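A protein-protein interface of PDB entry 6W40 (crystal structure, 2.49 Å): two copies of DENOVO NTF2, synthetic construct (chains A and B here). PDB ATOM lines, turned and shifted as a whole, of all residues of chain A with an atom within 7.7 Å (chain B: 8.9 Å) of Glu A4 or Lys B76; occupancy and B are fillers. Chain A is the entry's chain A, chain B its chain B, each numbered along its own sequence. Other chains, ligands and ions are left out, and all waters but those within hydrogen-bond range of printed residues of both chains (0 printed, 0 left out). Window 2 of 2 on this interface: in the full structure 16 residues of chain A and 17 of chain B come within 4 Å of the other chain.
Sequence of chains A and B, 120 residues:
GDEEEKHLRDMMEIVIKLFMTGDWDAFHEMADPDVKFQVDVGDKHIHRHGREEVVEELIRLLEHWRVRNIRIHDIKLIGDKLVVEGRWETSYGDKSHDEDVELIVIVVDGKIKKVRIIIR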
ATOM      1  N   GLY A   1       4.077   1.563  -9.670  1.00  0.00           N
ATOM      2  CA  GLY A   1       3.465   2.276  -8.565  1.00  0.00           C
ATOM      3  C   GLY A   1       2.999   3.667  -8.942  1.00  0.00           C
ATOM      4  O   GLY A   1       1.800   3.927  -9.024  1.00  0.00           O
ATOM      5  N   ASP A   2       3.960   4.565  -9.174  1.00  0.00           N
ATOM      6  CA  ASP A   2       3.631   5.936  -9.547  1.00  0.00           C
ATOM      7  C   ASP A   2       3.017   6.027 -10.937  1.00  0.00           C
ATOM      8  O   ASP A   2       2.286   6.983 -11.217  1.00  0.00           O
ATOM      9  CB  ASP A   2       4.882   6.813  -9.479  1.00  0.00           C
ATOM     10  CG  ASP A   2       5.631   6.663  -8.168  1.00  0.00           C
ATOM     11  OD1 ASP A   2       6.349   5.653  -8.004  1.00  0.00           O
ATOM     12  OD2 ASP A   2       5.503   7.553  -7.301  1.00  0.00           O
ATOM     13  N   GLU A   3       3.295   5.058 -11.810  1.00  0.00           N
ATOM     14  CA  GLU A   3       2.788   5.110 -13.176  1.00  0.00           C
ATOM     15  C   GLU A   3       1.298   4.793 -13.234  1.00  0.00           C
ATOM     16  O   GLU A   3       0.516   5.560 -13.806  1.00  0.00           O
ATOM     17  CB  GLU A   3       3.573   4.145 -14.066  1.00  0.00           C
ATOM     18  CG  GLU A   3       3.023   4.026 -15.476  1.00  0.00           C
ATOM     19  CD  GLU A   3       3.902   3.180 -16.372  1.00  0.00           C
ATOM     20  OE1 GLU A   3       5.089   2.991 -16.033  1.00  0.00           O
ATOM     21  OE2 GLU A   3       3.405   2.701 -17.414  1.00  0.00           O
ATOM     22  N   GLU A   4       0.887   3.663 -12.652  1.00  0.00           N
ATOM     23  CA  GLU A   4      -0.517   3.271 -12.730  1.00  0.00           C
ATOM     24  C   GLU A   4      -1.407   4.265 -11.997  1.00  0.00           C
ATOM     25  O   GLU A   4      -2.523   4.556 -12.443  1.00  0.00           O
ATOM     26  CB  GLU A   4      -0.714   1.865 -12.167  1.00  0.00           C
ATOM     27  CG  GLU A   4      -1.974   1.183 -12.682  1.00  0.00           C
ATOM     28  CD  GLU A   4      -2.448   0.057 -11.784  1.00  0.00           C
ATOM     29  OE1 GLU A   4      -3.563   0.170 -11.232  1.00  0.00           O
ATOM     30  OE2 GLU A   4      -1.707  -0.937 -11.628  1.00  0.00           O
ATOM     31  N   GLU A   5      -0.930   4.796 -10.868  1.00  0.00           N
ATOM     32  CA  GLU A   5      -1.687   5.813 -10.144  1.00  0.00           C
ATOM     33  C   GLU A   5      -1.968   7.018 -11.032  1.00  0.00           C
ATOM     34  O   GLU A   5      -3.099   7.513 -11.090  1.00  0.00           O
ATOM     35  CB  GLU A   5      -0.924   6.233  -8.888  1.00  0.00           C
ATOM     36  CG  GLU A   5      -1.570   7.373  -8.118  1.00  0.00           C
ATOM     37  CD  GLU A   5      -2.950   7.016  -7.602  1.00  0.00           C
ATOM     38  OE1 GLU A   5      -3.770   7.938  -7.410  1.00  0.00           O
ATOM     39  OE2 GLU A   5      -3.214   5.814  -7.390  1.00  0.00           O
ATOM     40  N   LYS A   6      -0.943   7.498 -11.740  1.00  0.00           N
ATOM     41  CA  LYS A   6      -1.129   8.607 -12.669  1.00  0.00           C
ATOM     42  C   LYS A   6      -2.157   8.262 -13.740  1.00  0.00           C
ATOM     43  O   LYS A   6      -2.963   9.113 -14.136  1.00  0.00           O
ATOM     44  CB  LYS A   6       0.214   8.980 -13.301  1.00  0.00           C
ATOM     45  CG  LYS A   6       0.119   9.869 -14.530  1.00  0.00           C
ATOM     46  CD  LYS A   6      -0.501  11.215 -14.208  1.00  0.00           C
ATOM     47  CE  LYS A   6      -0.584  12.076 -15.449  1.00  0.00           C
ATOM     48  NZ  LYS A   6      -1.178  11.327 -16.593  1.00  0.00           N
ATOM     49  N   HIS A   7      -2.155   7.013 -14.207  1.00  0.00           N
ATOM     50  CA  HIS A   7      -3.100   6.619 -15.245  1.00  0.00           C
ATOM     51  C   HIS A   7      -4.515   6.509 -14.693  1.00  0.00           C
ATOM     52  O   HIS A   7      -5.483   6.867 -15.376  1.00  0.00           O
ATOM     53  CB  HIS A   7      -2.666   5.299 -15.876  1.00  0.00           C
ATOM     54  CG  HIS A   7      -2.918   5.232 -17.346  1.00  0.00           C
ATOM     55  ND1 HIS A   7      -2.476   6.205 -18.217  1.00  0.00           N
ATOM     56  CD2 HIS A   7      -3.571   4.318 -18.102  1.00  0.00           C
ATOM     57  CE1 HIS A   7      -2.841   5.891 -19.447  1.00  0.00           C
ATOM     58  NE2 HIS A   7      -3.506   4.750 -19.404  1.00  0.00           N
ATOM     59  N   LEU A   8      -4.658   6.008 -13.463  1.00  0.00           N
ATOM     60  CA  LEU A   8      -5.964   5.997 -12.813  1.00  0.00           C
ATOM     61  C   LEU A   8      -6.516   7.409 -12.674  1.00  0.00           C
ATOM     62  O   LEU A   8      -7.722   7.633 -12.829  1.00  0.00           O
ATOM     63  CB  LEU A   8      -5.866   5.335 -11.441  1.00  0.00           C
ATOM     64  CG  LEU A   8      -6.172   3.844 -11.298  1.00  0.00           C
ATOM     65  CD1 LEU A   8      -5.257   3.001 -12.167  1.00  0.00           C
ATOM     66  CD2 LEU A   8      -6.044   3.445  -9.842  1.00  0.00           C
ATOM     67  N   ARG A   9      -5.642   8.373 -12.379  1.00  0.00           N
ATOM     68  CA  ARG A   9      -6.080   9.757 -12.246  1.00  0.00           C
ATOM     69  C   ARG A   9      -6.512  10.331 -13.588  1.00  0.00           C
ATOM     70  O   ARG A   9      -7.527  11.032 -13.670  1.00  0.00           O
ATOM     71  CB  ARG A   9      -4.964  10.596 -11.624  1.00  0.00           C
ATOM     72  CG  ARG A   9      -4.870  10.465 -10.111  1.00  0.00           C
ATOM     73  CD  ARG A   9      -3.439  10.240  -9.641  1.00  0.00           C
ATOM     74  NE  ARG A   9      -2.458  10.949 -10.458  1.00  0.00           N
ATOM     75  CZ  ARG A   9      -1.161  11.014 -10.172  1.00  0.00           C
ATOM     76  NH1 ARG A   9      -0.689  10.414  -9.088  1.00  0.00           N
ATOM     77  NH2 ARG A   9      -0.336  11.680 -10.970  1.00  0.00           N
ATOM     78  N   ASP A  10      -5.761  10.037 -14.654  1.00  0.00           N
ATOM     79  CA  ASP A  10      -6.125  10.524 -15.982  1.00  0.00           C
ATOM     80  C   ASP A  10      -7.520  10.054 -16.379  1.00  0.00           C
ATOM     81  O   ASP A  10      -8.347  10.850 -16.839  1.00  0.00           O
ATOM     82  CB  ASP A  10      -5.088  10.065 -17.010  1.00  0.00           C
ATOM     83  CG  ASP A  10      -4.199  11.198 -17.492  1.00  0.00           C
ATOM     84  OD1 ASP A  10      -4.689  12.341 -17.595  1.00  0.00           O
ATOM     85  OD2 ASP A  10      -3.008  10.946 -17.774  1.00  0.00           O
ATOM     86  N   ARG B   9      -0.707   0.280 -24.449  1.00  0.00           N
ATOM     87  CA  ARG B   9      -1.471   0.747 -23.299  1.00  0.00           C
ATOM     88  C   ARG B   9      -2.347   1.938 -23.671  1.00  0.00           C
ATOM     89  O   ARG B   9      -3.547   1.955 -23.380  1.00  0.00           O
ATOM     90  CB  ARG B   9      -0.524   1.113 -22.157  1.00  0.00           C
ATOM     91  CG  ARG B   9      -1.215   1.730 -20.957  1.00  0.00           C
ATOM     92  CD  ARG B   9      -0.207   2.400 -20.041  1.00  0.00           C
ATOM     93  NE  ARG B   9       0.589   3.393 -20.758  1.00  0.00           N
ATOM     94  CZ  ARG B   9       1.465   4.208 -20.182  1.00  0.00           C
ATOM     95  NH1 ARG B   9       1.661   4.155 -18.872  1.00  0.00           N
ATOM     96  NH2 ARG B   9       2.144   5.080 -20.916  1.00  0.00           N
ATOM     97  N   MET B  12      -5.267   0.899 -26.046  1.00  0.00           N
ATOM     98  CA  MET B  12      -6.351   0.227 -25.336  1.00  0.00           C
ATOM     99  C   MET B  12      -7.146   1.211 -24.490  1.00  0.00           C
ATOM    100  O   MET B  12      -8.372   1.094 -24.373  1.00  0.00           O
ATOM    101  CB  MET B  12      -5.792  -0.902 -24.471  1.00  0.00           C
ATOM    102  CG  MET B  12      -5.138  -2.024 -25.262  1.00  0.00           C
ATOM    103  SD  MET B  12      -6.269  -2.788 -26.439  1.00  0.00           S
ATOM    104  CE  MET B  12      -5.178  -3.942 -27.265  1.00  0.00           C
ATOM    105  N   GLU B  13      -6.467   2.195 -23.897  1.00  0.00           N
ATOM    106  CA  GLU B  13      -7.163   3.189 -23.088  1.00  0.00           C
ATOM    107  C   GLU B  13      -8.003   4.116 -23.954  1.00  0.00           C
ATOM    108  O   GLU B  13      -9.144   4.438 -23.603  1.00  0.00           O
ATOM    109  CB  GLU B  13      -6.157   3.988 -22.266  1.00  0.00           C
ATOM    110  CG  GLU B  13      -5.449   3.159 -21.219  1.00  0.00           C
ATOM    111  CD  GLU B  13      -6.276   2.974 -19.968  1.00  0.00           C
ATOM    112  OE1 GLU B  13      -6.936   3.945 -19.546  1.00  0.00           O
ATOM    113  OE2 GLU B  13      -6.270   1.856 -19.410  1.00  0.00           O
ATOM    114  N   ILE B  16     -11.220   2.493 -24.829  1.00  0.00           N
ATOM    115  CA  ILE B  16     -12.234   2.504 -23.778  1.00  0.00           C
ATOM    116  C   ILE B  16     -12.952   3.843 -23.741  1.00  0.00           C
ATOM    117  O   ILE B  16     -14.163   3.908 -23.494  1.00  0.00           O
ATOM    118  CB  ILE B  16     -11.599   2.171 -22.417  1.00  0.00           C
ATOM    119  CG1 ILE B  16     -10.884   0.826 -22.492  1.00  0.00           C
ATOM    120  CG2 ILE B  16     -12.655   2.139 -21.325  1.00  0.00           C
ATOM    121  CD1 ILE B  16     -11.732  -0.272 -23.070  1.00  0.00           C
ATOM    122  N   ILE B  72     -11.833   5.217 -10.352  1.00  0.00           N
ATOM    123  CA  ILE B  72     -11.030   4.142 -10.925  1.00  0.00           C
ATOM    124  C   ILE B  72     -10.075   3.632  -9.854  1.00  0.00           C
ATOM    125  O   ILE B  72      -9.257   4.394  -9.324  1.00  0.00           O
ATOM    126  CB  ILE B  72     -10.268   4.614 -12.173  1.00  0.00           C
ATOM    127  CG1 ILE B  72     -11.228   5.274 -13.164  1.00  0.00           C
ATOM    128  CG2 ILE B  72      -9.559   3.442 -12.837  1.00  0.00           C
ATOM    129  CD1 ILE B  72     -12.348   4.368 -13.629  1.00  0.00           C
ATOM    130  N   HIS B  73     -10.173   2.341  -9.536  1.00  0.00           N
ATOM    131  CA  HIS B  73      -9.357   1.732  -8.493  1.00  0.00           C
ATOM    132  C   HIS B  73      -8.189   0.918  -9.029  1.00  0.00           C
ATOM    133  O   HIS B  73      -7.165   0.808  -8.345  1.00  0.00           O
ATOM    134  CB  HIS B  73     -10.216   0.827  -7.602  1.00  0.00           C
ATOM    135  CG  HIS B  73     -11.178   1.572  -6.731  1.00  0.00           C
ATOM    136  ND1 HIS B  73     -11.129   2.939  -6.566  1.00  0.00           N
ATOM    137  CD2 HIS B  73     -12.215   1.138  -5.975  1.00  0.00           C
ATOM    138  CE1 HIS B  73     -12.095   3.315  -5.745  1.00  0.00           C
ATOM    139  NE2 HIS B  73     -12.768   2.241  -5.374  1.00  0.00           N
ATOM    140  N   ASP B  74      -8.308   0.341 -10.223  1.00  0.00           N
ATOM    141  CA  ASP B  74      -7.256  -0.522 -10.742  1.00  0.00           C
ATOM    142  C   ASP B  74      -7.357  -0.584 -12.259  1.00  0.00           C
ATOM    143  O   ASP B  74      -8.458  -0.655 -12.811  1.00  0.00           O
ATOM    144  CB  ASP B  74      -7.353  -1.931 -10.142  1.00  0.00           C
ATOM    145  CG  ASP B  74      -6.151  -2.797 -10.477  1.00  0.00           C
ATOM    146  OD1 ASP B  74      -5.181  -2.278 -11.070  1.00  0.00           O
ATOM    147  OD2 ASP B  74      -6.177  -4.001 -10.145  1.00  0.00           O
ATOM    148  N   ILE B  75      -6.201  -0.551 -12.920  1.00  0.00           N
ATOM    149  CA  ILE B  75      -6.097  -0.715 -14.366  1.00  0.00           C
ATOM    150  C   ILE B  75      -4.951  -1.675 -14.645  1.00  0.00           C
ATOM    151  O   ILE B  75      -3.836  -1.476 -14.150  1.00  0.00           O
ATOM    152  CB  ILE B  75      -5.865   0.627 -15.088  1.00  0.00           C
ATOM    153  CG1 ILE B  75      -7.068   1.556 -14.917  1.00  0.00           C
ATOM    154  CG2 ILE B  75      -5.590   0.398 -16.565  1.00  0.00           C
ATOM    155  CD1 ILE B  75      -6.878   2.920 -15.548  1.00  0.00           C
ATOM    156  N   LYS B  76      -5.225  -2.718 -15.427  1.00  0.00           N
ATOM    157  CA  LYS B  76      -4.218  -3.714 -15.772  1.00  0.00           C
ATOM    158  C   LYS B  76      -4.305  -4.030 -17.256  1.00  0.00           C
ATOM    159  O   LYS B  76      -5.394  -4.292 -17.776  1.00  0.00           O
ATOM    160  CB  LYS B  76      -4.399  -4.995 -14.950  1.00  0.00           C
ATOM    161  CG  LYS B  76      -3.862  -4.908 -13.532  1.00  0.00           C
ATOM    162  CD  LYS B  76      -2.349  -4.763 -13.527  1.00  0.00           C
ATOM    163  CE  LYS B  76      -1.793  -4.795 -12.112  1.00  0.00           C
ATOM    164  NZ  LYS B  76      -2.368  -3.714 -11.264  1.00  0.00           N
ATOM    165  N   LEU B  77      -3.158  -4.009 -17.929  1.00  0.00           N
ATOM    166  CA  LEU B  77      -3.057  -4.338 -19.346  1.00  0.00           C
ATOM    167  C   LEU B  77      -2.308  -5.660 -19.463  1.00  0.00           C
ATOM    168  O   LEU B  77      -1.115  -5.735 -19.154  1.00  0.00           O
ATOM    169  CB  LEU B  77      -2.352  -3.220 -20.115  1.00  0.00           C
ATOM    170  CG  LEU B  77      -2.321  -3.273 -21.648  1.00  0.00           C
ATOM    171  CD1 LEU B  77      -1.094  -4.016 -22.155  1.00  0.00           C
ATOM    172  CD2 LEU B  77      -3.596  -3.901 -22.201  1.00  0.00           C
ATOM    173  N   ILE B  78      -3.013  -6.703 -19.901  1.00  0.00           N
ATOM    174  CA  ILE B  78      -2.431  -8.035 -20.020  1.00  0.00           C
ATOM    175  C   ILE B  78      -2.575  -8.522 -21.457  1.00  0.00           C
ATOM    176  O   ILE B  78      -3.489  -9.289 -21.777  1.00  0.00           O
ATOM    177  CB  ILE B  78      -3.093  -9.020 -19.039  1.00  0.00           C
ATOM    178  CG1 ILE B  78      -3.282  -8.361 -17.670  1.00  0.00           C
ATOM    179  CG2 ILE B  78      -2.257 -10.282 -18.908  1.00  0.00           C
ATOM    180  CD1 ILE B  78      -4.133  -9.164 -16.717  1.00  0.00           C
ATOM    181  N   GLY B  79      -1.673  -8.083 -22.330  1.00  0.00           N
ATOM    182  CA  GLY B  79      -1.730  -8.475 -23.725  1.00  0.00           C
ATOM    183  C   GLY B  79      -2.873  -7.822 -24.472  1.00  0.00           C
ATOM    184  O   GLY B  79      -2.899  -6.599 -24.631  1.00  0.00           O
ATOM    185  N   ASP B  80      -3.830  -8.625 -24.929  1.00  0.00           N
ATOM    186  CA  ASP B  80      -4.980  -8.120 -25.668  1.00  0.00           C
ATOM    187  C   ASP B  80      -6.168  -7.790 -24.775  1.00  0.00           C
ATOM    188  O   ASP B  80      -7.212  -7.371 -25.286  1.00  0.00           O
ATOM    189  CB  ASP B  80      -5.405  -9.131 -26.740  1.00  0.00           C
ATOM    190  CG  ASP B  80      -5.785 -10.484 -26.157  1.00  0.00           C
ATOM    191  OD1 ASP B  80      -5.616 -10.686 -24.936  1.00  0.00           O
ATOM    192  OD2 ASP B  80      -6.255 -11.349 -26.927  1.00  0.00           O
ATOM    193  N   LYS B  81      -6.040  -7.963 -23.462  1.00  0.00           N
ATOM    194  CA  LYS B  81      -7.136  -7.755 -22.525  1.00  0.00           C
ATOM    195  C   LYS B  81      -6.810  -6.592 -21.600  1.00  0.00           C
ATOM    196  O   LYS B  81      -5.694  -6.501 -21.078  1.00  0.00           O
ATOM    197  CB  LYS B  81      -7.403  -9.023 -21.706  1.00  0.00           C
ATOM    198  CG  LYS B  81      -8.339  -8.817 -20.524  1.00  0.00           C
ATOM    199  CD  LYS B  81      -8.805 -10.145 -19.949  1.00  0.00           C
ATOM    200  CE  LYS B  81      -7.633 -11.005 -19.512  1.00  0.00           C
ATOM    201  NZ  LYS B  81      -8.087 -12.319 -18.978  1.00  0.00           N
ATOM    202  N   LEU B  82      -7.785  -5.709 -21.401  1.00  0.00           N
ATOM    203  CA  LEU B  82      -7.683  -4.617 -20.441  1.00  0.00           C
ATOM    204  C   LEU B  82      -8.726  -4.825 -19.354  1.00  0.00           C
ATOM    205  O   LEU B  82      -9.906  -5.037 -19.655  1.00  0.00           O
ATOM    206  CB  LEU B  82      -7.881  -3.259 -21.119  1.00  0.00           C
ATOM    207  CG  LEU B  82      -7.672  -2.035 -20.223  1.00  0.00           C
ATOM    208  CD1 LEU B  82      -6.211  -1.904 -19.820  1.00  0.00           C
ATOM    209  CD2 LEU B  82      -8.152  -0.772 -20.908  1.00  0.00           C
ATOM    210  N   VAL B  83      -8.293  -4.770 -18.098  1.00  0.00           N
ATOM    211  CA  VAL B  83      -9.166  -4.971 -16.946  1.00  0.00           C
ATOM    212  C   VAL B  83      -9.157  -3.694 -16.119  1.00  0.00           C
ATOM    213  O   VAL B  83      -8.095  -3.245 -15.669  1.00  0.00           O
ATOM    214  CB  VAL B  83      -8.730  -6.176 -16.097  1.00  0.00           C
ATOM    215  CG1 VAL B  83      -9.639  -6.324 -14.888  1.00  0.00           C
ATOM    216  CG2 VAL B  83      -8.738  -7.447 -16.931  1.00  0.00           C
ATOM    217  N   VAL B  84     -10.336  -3.110 -15.922  1.00  0.00           N
ATOM    218  CA  VAL B  84     -10.503  -1.897 -15.132  1.00  0.00           C
ATOM    219  C   VAL B  84     -11.472  -2.198 -13.999  1.00  0.00           C
ATOM    220  O   VAL B  84     -12.572  -2.710 -14.235  1.00  0.00           O
ATOM    221  CB  VAL B  84     -11.015  -0.724 -15.990  1.00  0.00           C
ATOM    222  CG1 VAL B  84     -11.154   0.534 -15.143  1.00  0.00           C
ATOM    223  CG2 VAL B  84     -10.086  -0.478 -17.170  1.00  0.00           C
ATOM    224  N   GLU B  85     -11.062  -1.882 -12.772  1.00  0.00           N
ATOM    225  CA  GLU B  85     -11.893  -2.054 -11.589  1.00  0.00           C
ATOM    226  C   GLU B  85     -12.125  -0.696 -10.946  1.00  0.00           C
ATOM    227  O   GLU B  85     -11.186   0.092 -10.795  1.00  0.00           O
ATOM    228  CB  GLU B  85     -11.240  -3.013 -10.591  1.00  0.00           C
ATOM    229  CG  GLU B  85     -10.979  -4.389 -11.163  1.00  0.00           C
ATOM    230  CD  GLU B  85     -10.505  -5.375 -10.119  1.00  0.00           C
ATOM    231  OE1 GLU B  85      -9.894  -4.940  -9.121  1.00  0.00           O
ATOM    232  OE2 GLU B  85     -10.752  -6.587 -10.297  1.00  0.00           O
ATOM    233  N   LEU B 103     -14.640  -3.582 -15.438  1.00  0.00           N
ATOM    234  CA  LEU B 103     -14.737  -3.486 -16.886  1.00  0.00           C
ATOM    235  C   LEU B 103     -13.627  -4.308 -17.524  1.00  0.00           C
ATOM    236  O   LEU B 103     -12.450  -4.128 -17.198  1.00  0.00           O
ATOM    237  CB  LEU B 103     -14.648  -2.032 -17.352  1.00  0.00           C
ATOM    238  CG  LEU B 103     -14.646  -1.840 -18.871  1.00  0.00           C
ATOM    239  CD1 LEU B 103     -15.943  -2.351 -19.483  1.00  0.00           C
ATOM    240  CD2 LEU B 103     -14.415  -0.382 -19.230  1.00  0.00           C
ATOM    241  N   ILE B 104     -14.008  -5.206 -18.429  1.00  0.00           N
ATOM    242  CA  ILE B 104     -13.071  -6.072 -19.134  1.00  0.00           C
ATOM    243  C   ILE B 104     -13.321  -5.922 -20.627  1.00  0.00           C
ATOM    244  O   ILE B 104     -14.453  -6.096 -21.092  1.00  0.00           O
ATOM    245  CB  ILE B 104     -13.220  -7.543 -18.705  1.00  0.00           C
ATOM    246  CG1 ILE B 104     -13.029  -7.668 -17.194  1.00  0.00           C
ATOM    247  CG2 ILE B 104     -12.224  -8.420 -19.451  1.00  0.00           C
ATOM    248  CD1 ILE B 104     -13.640  -8.908 -16.606  1.00  0.00           C
ATOM    249  N   VAL B 105     -12.271  -5.594 -21.374  1.00  0.00           N
ATOM    250  CA  VAL B 105     -12.360  -5.399 -22.814  1.00  0.00           C
ATOM    251  C   VAL B 105     -11.189  -6.110 -23.473  1.00  0.00           C
ATOM    252  O   VAL B 105     -10.030  -5.877 -23.110  1.00  0.00           O
ATOM    253  CB  VAL B 105     -12.371  -3.905 -23.191  1.00  0.00           C
ATOM    254  CG1 VAL B 105     -12.216  -3.736 -24.692  1.00  0.00           C
ATOM    255  CG2 VAL B 105     -13.660  -3.253 -22.712  1.00  0.00           C
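The guanidinium group (NH1) of Arg B9 lies within salt-bridge range of the side-chain carboxylate (OE2) of Glu A3 (2.7 Å). OE1 of Glu A4 lies within hydrogen-bond range of N of Ile B75 (3.2 Å). The side-chain amino group (NZ) of Lys B76 is in salt-bridge range of the side-chain carboxylate (OE2) of Glu A4, 2.9 Å away. The side-chain carboxylate (OE1) of Glu A4 sits close to the side-chain carboxylate (OD1) of Asp B74 (2.9 Å).
The backbone NH of His B73 lies within hydrogen-bond range of the backbone carbonyl oxygen of Glu B85 (2.8 Å). The side-chain carboxylate (OD1) of Asp B74 is in salt-bridge range of the side-chain amino group (NZ) of Lys B76. N of Glu B85 lies within hydrogen-bond range of O of Asp B74 (2.9 Å). The backbone NH of Lys B76 sits at hydrogen-bond distance from the backbone carbonyl oxygen of Val B83 (2.9 Å).
His A7 touches Glu B13. Leu A8 touches Ile B72. His B73 touches Leu A8 (O to CD2, 3.2 Å). Leu A8 touches Asp B74. CD1 of Leu A8 touches CG1 of Ile B75, at 3.6 Å.
Glu A4 touches just these residues of chain B: Asp B74 (2.9 Å), Ile B75 (3.1 Å) and Lys B76 (2.9 Å). Of the printed residues of chain B, His A7 touches Glu B13 (3.1 Å). Of the printed residues of chain A, Glu B13 touches His A7. Of chain A, only Glu A4 comes within 4 Å of Lys B76. Leu B103 touches none of the printed residues of chain A. The nearest residue of chain B that does not touch Glu A4 is His B73 (4.7 Å). The nearest printed residue of chain A that does not touch Asp B74 is Glu A5 (8.0 Å).
Of the 10 printed residues of chain A, 4 touch a printed residue of chain B. Printed residues of chain B that touch a printed residue of chain A: Arg B9, Glu B13, Ile B72, His B73, Asp B74, Ile B75 and Lys B76. Among the printed residues, 9 pairs touch across the chains.
Position printed for both chains: 9.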
